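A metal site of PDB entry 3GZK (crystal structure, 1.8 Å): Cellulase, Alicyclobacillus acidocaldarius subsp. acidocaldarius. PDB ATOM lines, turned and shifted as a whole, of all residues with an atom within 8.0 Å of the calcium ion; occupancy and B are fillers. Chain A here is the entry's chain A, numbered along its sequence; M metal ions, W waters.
The side-chain carboxylate of Asp 307 sits close to the backbone NH of Val 346 (2.9 Å). OE1 of Glu 304 is in salt-bridge range of NH2 of Arg 306, at 2.9 Å.
Of the 20 residues printed, 5 come within 4 Å of the calcium ion. The nearest printed residue that does not touch the calcium ion is Asp 345 (4.4 Å).
OD2 of Asp 302 binds the calcium ion. O of Ala 344 is bound to the calcium ion, 2.4 Å away. The calcium ion is bound by OE2 of Glu 308 (2.4 Å). O of Glu 304 is bound to the calcium ion (2.5 Å). Water W1 binds the calcium ion (2.5 Å). The side-chain carboxylate (OD2) of Asp 307 binds the calcium ion (2.5 Å). The calcium ion is bound by the side-chain carboxylate (OE1) of Glu 308, 2.5 Å away. The side-chain carboxylate (OD1) of Asp 307 is bound to the calcium ion. The calcium ion has eight donor atoms within binding distance.
Water W1 lies within hydrogen-bond range of the side-chain carboxylate of Asp 345 (2.7 Å) and the side-chain carboxylate of Asp 302 (2.8 Å).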
ATOM      1  N   VAL A 152     -22.489  29.013 -28.063  1.00  0.00           N
ATOM      2  CA  VAL A 152     -21.734  28.024 -27.285  1.00  0.00           C
ATOM      3  C   VAL A 152     -22.233  27.893 -25.824  1.00  0.00           C
ATOM      4  O   VAL A 152     -22.605  26.785 -25.415  1.00  0.00           O
ATOM      5  CB  VAL A 152     -20.213  28.274 -27.379  1.00  0.00           C
ATOM      6  CG1 VAL A 152     -19.417  27.385 -26.419  1.00  0.00           C
ATOM      7  CG2 VAL A 152     -19.763  28.061 -28.808  1.00  0.00           C
ATOM      8  N   ALA A 243     -17.166  25.499 -33.148  1.00  0.00           N
ATOM      9  CA  ALA A 243     -17.652  25.330 -31.774  1.00  0.00           C
ATOM     10  C   ALA A 243     -19.159  25.542 -31.675  1.00  0.00           C
ATOM     11  O   ALA A 243     -19.851  24.733 -31.074  1.00  0.00           O
ATOM     12  CB  ALA A 243     -16.906  26.242 -30.806  1.00  0.00           C
ATOM     13  N   THR A 247     -21.776  22.415 -30.774  1.00  0.00           N
ATOM     14  CA  THR A 247     -22.559  22.511 -29.542  1.00  0.00           C
ATOM     15  C   THR A 247     -24.055  22.666 -29.852  1.00  0.00           C
ATOM     16  O   THR A 247     -24.888  22.101 -29.165  1.00  0.00           O
ATOM     17  CB  THR A 247     -22.086  23.650 -28.605  1.00  0.00           C
ATOM     18  OG1 THR A 247     -22.103  24.900 -29.305  1.00  0.00           O
ATOM     19  CG2 THR A 247     -20.689  23.365 -28.064  1.00  0.00           C
ATOM     20  N   GLY A 301     -14.248  31.962 -26.994  1.00  0.00           N
ATOM     21  CA  GLY A 301     -13.298  31.250 -27.822  1.00  0.00           C
ATOM     22  C   GLY A 301     -12.872  29.965 -27.145  1.00  0.00           C
ATOM     23  O   GLY A 301     -13.202  29.729 -25.989  1.00  0.00           O
ATOM     24  N   ASP A 302     -12.141  29.141 -27.877  1.00  0.00           N
ATOM     25  CA  ASP A 302     -11.750  27.821 -27.388  1.00  0.00           C
ATOM     26  C   ASP A 302     -10.852  27.164 -28.436  1.00  0.00           C
ATOM     27  O   ASP A 302     -11.254  27.019 -29.590  1.00  0.00           O
ATOM     28  CB  ASP A 302     -13.000  26.972 -27.152  1.00  0.00           C
ATOM     29  CG  ASP A 302     -12.685  25.596 -26.600  1.00  0.00           C
ATOM     30  OD1 ASP A 302     -11.579  25.370 -26.061  1.00  0.00           O
ATOM     31  OD2 ASP A 302     -13.580  24.726 -26.734  1.00  0.00           O
ATOM     32  N   ALA A 303      -9.648  26.776 -28.019  1.00  0.00           N
ATOM     33  CA  ALA A 303      -8.671  26.187 -28.937  1.00  0.00           C
ATOM     34  C   ALA A 303      -8.840  24.682 -29.128  1.00  0.00           C
ATOM     35  O   ALA A 303      -8.408  24.132 -30.149  1.00  0.00           O
ATOM     36  CB  ALA A 303      -7.244  26.506 -28.453  1.00  0.00           C
ATOM     37  N   GLU A 304      -9.474  24.018 -28.169  1.00  0.00           N
ATOM     38  CA  GLU A 304      -9.669  22.563 -28.232  1.00  0.00           C
ATOM     39  C   GLU A 304     -11.110  22.254 -28.639  1.00  0.00           C
ATOM     40  O   GLU A 304     -12.028  22.598 -27.921  1.00  0.00           O
ATOM     41  CB  GLU A 304      -9.363  21.934 -26.870  1.00  0.00           C
ATOM     42  CG  GLU A 304      -9.637  20.437 -26.798  1.00  0.00           C
ATOM     43  CD  GLU A 304      -8.851  19.672 -27.843  1.00  0.00           C
ATOM     44  OE1 GLU A 304      -7.622  19.598 -27.704  1.00  0.00           O
ATOM     45  OE2 GLU A 304      -9.474  19.169 -28.798  1.00  0.00           O
ATOM     46  N   LEU A 305     -11.292  21.634 -29.801  1.00  0.00           N
ATOM     47  CA  LEU A 305     -12.644  21.391 -30.312  1.00  0.00           C
ATOM     48  C   LEU A 305     -13.036  19.915 -30.410  1.00  0.00           C
ATOM     49  O   LEU A 305     -14.141  19.602 -30.837  1.00  0.00           O
ATOM     50  CB  LEU A 305     -12.839  22.098 -31.665  1.00  0.00           C
ATOM     51  CG  LEU A 305     -12.688  23.625 -31.589  1.00  0.00           C
ATOM     52  CD1 LEU A 305     -12.732  24.259 -32.990  1.00  0.00           C
ATOM     53  CD2 LEU A 305     -13.770  24.225 -30.685  1.00  0.00           C
ATOM     54  N   ARG A 306     -12.159  18.997 -30.008  1.00  0.00           N
ATOM     55  CA  ARG A 306     -12.465  17.572 -30.125  1.00  0.00           C
ATOM     56  C   ARG A 306     -13.551  17.143 -29.138  1.00  0.00           C
ATOM     57  O   ARG A 306     -14.318  16.236 -29.429  1.00  0.00           O
ATOM     58  CB  ARG A 306     -11.211  16.697 -29.971  1.00  0.00           C
ATOM     59  CG  ARG A 306     -10.273  16.831 -31.167  1.00  0.00           C
ATOM     60  CD  ARG A 306      -8.965  16.120 -30.927  1.00  0.00           C
ATOM     61  NE  ARG A 306      -8.188  16.793 -29.889  1.00  0.00           N
ATOM     62  CZ  ARG A 306      -7.079  16.321 -29.338  1.00  0.00           C
ATOM     63  NH1 ARG A 306      -6.573  15.161 -29.714  1.00  0.00           N
ATOM     64  NH2 ARG A 306      -6.467  17.024 -28.396  1.00  0.00           N
ATOM     65  N   ASP A 307     -13.611  17.810 -27.984  1.00  0.00           N
ATOM     66  CA  ASP A 307     -14.680  17.549 -27.004  1.00  0.00           C
ATOM     67  C   ASP A 307     -16.047  17.977 -27.545  1.00  0.00           C
ATOM     68  O   ASP A 307     -17.056  17.329 -27.259  1.00  0.00           O
ATOM     69  CB  ASP A 307     -14.368  18.166 -25.627  1.00  0.00           C
ATOM     70  CG  ASP A 307     -14.034  19.651 -25.697  1.00  0.00           C
ATOM     71  OD1 ASP A 307     -12.976  20.018 -26.265  1.00  0.00           O
ATOM     72  OD2 ASP A 307     -14.799  20.470 -25.143  1.00  0.00           O
ATOM     73  N   GLU A 308     -16.090  19.051 -28.332  1.00  0.00           N
ATOM     74  CA  GLU A 308     -17.330  19.462 -29.016  1.00  0.00           C
ATOM     75  C   GLU A 308     -17.770  18.409 -30.040  1.00  0.00           C
ATOM     76  O   GLU A 308     -18.947  18.068 -30.130  1.00  0.00           O
ATOM     77  CB  GLU A 308     -17.183  20.836 -29.694  1.00  0.00           C
ATOM     78  CG  GLU A 308     -17.259  22.018 -28.739  1.00  0.00           C
ATOM     79  CD  GLU A 308     -16.008  22.193 -27.901  1.00  0.00           C
ATOM     80  OE1 GLU A 308     -14.974  21.568 -28.209  1.00  0.00           O
ATOM     81  OE2 GLU A 308     -16.034  22.957 -26.928  1.00  0.00           O
ATOM     82  N   LEU A 309     -16.821  17.892 -30.816  1.00  0.00           N
ATOM     83  CA  LEU A 309     -17.121  16.825 -31.778  1.00  0.00           C
ATOM     84  C   LEU A 309     -17.584  15.571 -31.022  1.00  0.00           C
ATOM     85  O   LEU A 309     -18.543  14.911 -31.428  1.00  0.00           O
ATOM     86  CB  LEU A 309     -15.905  16.507 -32.652  1.00  0.00           C
ATOM     87  CG  LEU A 309     -16.081  15.383 -33.673  1.00  0.00           C
ATOM     88  CD1 LEU A 309     -17.261  15.634 -34.626  1.00  0.00           C
ATOM     89  CD2 LEU A 309     -14.788  15.204 -34.446  1.00  0.00           C
ATOM     90  N   LEU A 337      -8.986  14.032 -23.042  1.00  0.00           N
ATOM     91  CA  LEU A 337      -9.699  15.287 -22.856  1.00  0.00           C
ATOM     92  C   LEU A 337     -10.221  15.381 -21.417  1.00  0.00           C
ATOM     93  O   LEU A 337     -10.556  14.364 -20.822  1.00  0.00           O
ATOM     94  CB  LEU A 337     -10.888  15.366 -23.802  1.00  0.00           C
ATOM     95  CG  LEU A 337     -10.604  15.436 -25.299  1.00  0.00           C
ATOM     96  CD1 LEU A 337     -11.888  15.255 -26.105  1.00  0.00           C
ATOM     97  CD2 LEU A 337      -9.958  16.765 -25.640  1.00  0.00           C
ATOM     98  N   PRO A 338     -10.286  16.608 -20.859  1.00  0.00           N
ATOM     99  CA  PRO A 338     -10.959  16.747 -19.570  1.00  0.00           C
ATOM    100  C   PRO A 338     -12.441  16.414 -19.726  1.00  0.00           C
ATOM    101  O   PRO A 338     -13.057  16.792 -20.726  1.00  0.00           O
ATOM    102  CB  PRO A 338     -10.751  18.222 -19.220  1.00  0.00           C
ATOM    103  CG  PRO A 338     -10.501  18.896 -20.516  1.00  0.00           C
ATOM    104  CD  PRO A 338      -9.809  17.893 -21.376  1.00  0.00           C
ATOM    105  N   GLY A 342     -18.548  22.132 -19.430  1.00  0.00           N
ATOM    106  CA  GLY A 342     -18.601  23.381 -20.187  1.00  0.00           C
ATOM    107  C   GLY A 342     -18.311  24.642 -19.392  1.00  0.00           C
ATOM    108  O   GLY A 342     -17.915  24.570 -18.225  1.00  0.00           O
ATOM    109  N   TRP A 343     -18.488  25.814 -20.001  1.00  0.00           N
ATOM    110  CA  TRP A 343     -18.971  25.935 -21.379  1.00  0.00           C
ATOM    111  C   TRP A 343     -17.962  25.542 -22.473  1.00  0.00           C
ATOM    112  O   TRP A 343     -18.349  25.200 -23.582  1.00  0.00           O
ATOM    113  CB  TRP A 343     -19.492  27.358 -21.649  1.00  0.00           C
ATOM    114  CG  TRP A 343     -18.501  28.438 -21.402  1.00  0.00           C
ATOM    115  CD1 TRP A 343     -18.383  29.189 -20.269  1.00  0.00           C
ATOM    116  CD2 TRP A 343     -17.472  28.899 -22.301  1.00  0.00           C
ATOM    117  NE1 TRP A 343     -17.344  30.093 -20.402  1.00  0.00           N
ATOM    118  CE2 TRP A 343     -16.773  29.938 -21.639  1.00  0.00           C
ATOM    119  CE3 TRP A 343     -17.078  28.545 -23.604  1.00  0.00           C
ATOM    120  CZ2 TRP A 343     -15.703  30.612 -22.227  1.00  0.00           C
ATOM    121  CZ3 TRP A 343     -16.015  29.226 -24.182  1.00  0.00           C
ATOM    122  CH2 TRP A 343     -15.342  30.252 -23.497  1.00  0.00           C
ATOM    123  N   ALA A 344     -16.656  25.601 -22.153  1.00  0.00           N
ATOM    124  CA  ALA A 344     -15.582  25.342 -23.119  1.00  0.00           C
ATOM    125  C   ALA A 344     -15.176  23.872 -23.223  1.00  0.00           C
ATOM    126  O   ALA A 344     -14.851  23.386 -24.323  1.00  0.00           O
ATOM    127  CB  ALA A 344     -14.355  26.200 -22.789  1.00  0.00           C
ATOM    128  N   ASP A 345     -15.175  23.167 -22.092  1.00  0.00           N
ATOM    129  CA  ASP A 345     -14.743  21.787 -21.996  1.00  0.00           C
ATOM    130  C   ASP A 345     -15.973  20.952 -21.715  1.00  0.00           C
ATOM    131  O   ASP A 345     -16.412  20.842 -20.565  1.00  0.00           O
ATOM    132  CB  ASP A 345     -13.674  21.639 -20.906  1.00  0.00           C
ATOM    133  CG  ASP A 345     -12.460  22.510 -21.176  1.00  0.00           C
ATOM    134  OD1 ASP A 345     -12.297  23.541 -20.490  1.00  0.00           O
ATOM    135  OD2 ASP A 345     -11.701  22.201 -22.117  1.00  0.00           O
ATOM    136  N   VAL A 346     -16.522  20.356 -22.771  1.00  0.00           N
ATOM    137  CA  VAL A 346     -17.882  19.805 -22.743  1.00  0.00           C
ATOM    138  C   VAL A 346     -17.957  18.279 -22.826  1.00  0.00           C
ATOM    139  O   VAL A 346     -19.049  17.738 -22.985  1.00  0.00           O
ATOM    140  CB  VAL A 346     -18.732  20.391 -23.898  1.00  0.00           C
ATOM    141  CG1 VAL A 346     -18.972  21.878 -23.672  1.00  0.00           C
ATOM    142  CG2 VAL A 346     -18.061  20.128 -25.268  1.00  0.00           C
ATOM    143  N   ALA A 347     -16.818  17.597 -22.714  1.00  0.00           N
ATOM    144  CA  ALA A 347     -16.756  16.152 -22.950  1.00  0.00           C
ATOM    145  C   ALA A 347     -17.691  15.305 -22.079  1.00  0.00           C
ATOM    146  O   ALA A 347     -18.199  14.309 -22.547  1.00  0.00           O
ATOM    147  CB  ALA A 347     -15.325  15.639 -22.809  1.00  0.00           C
HETATM  148 CA    CA M   1     -13.778  22.471 -26.211  1.00  0.00          CA
HETATM  149  O   HOH W   1     -11.873  22.954 -24.732  1.00  0.00           O
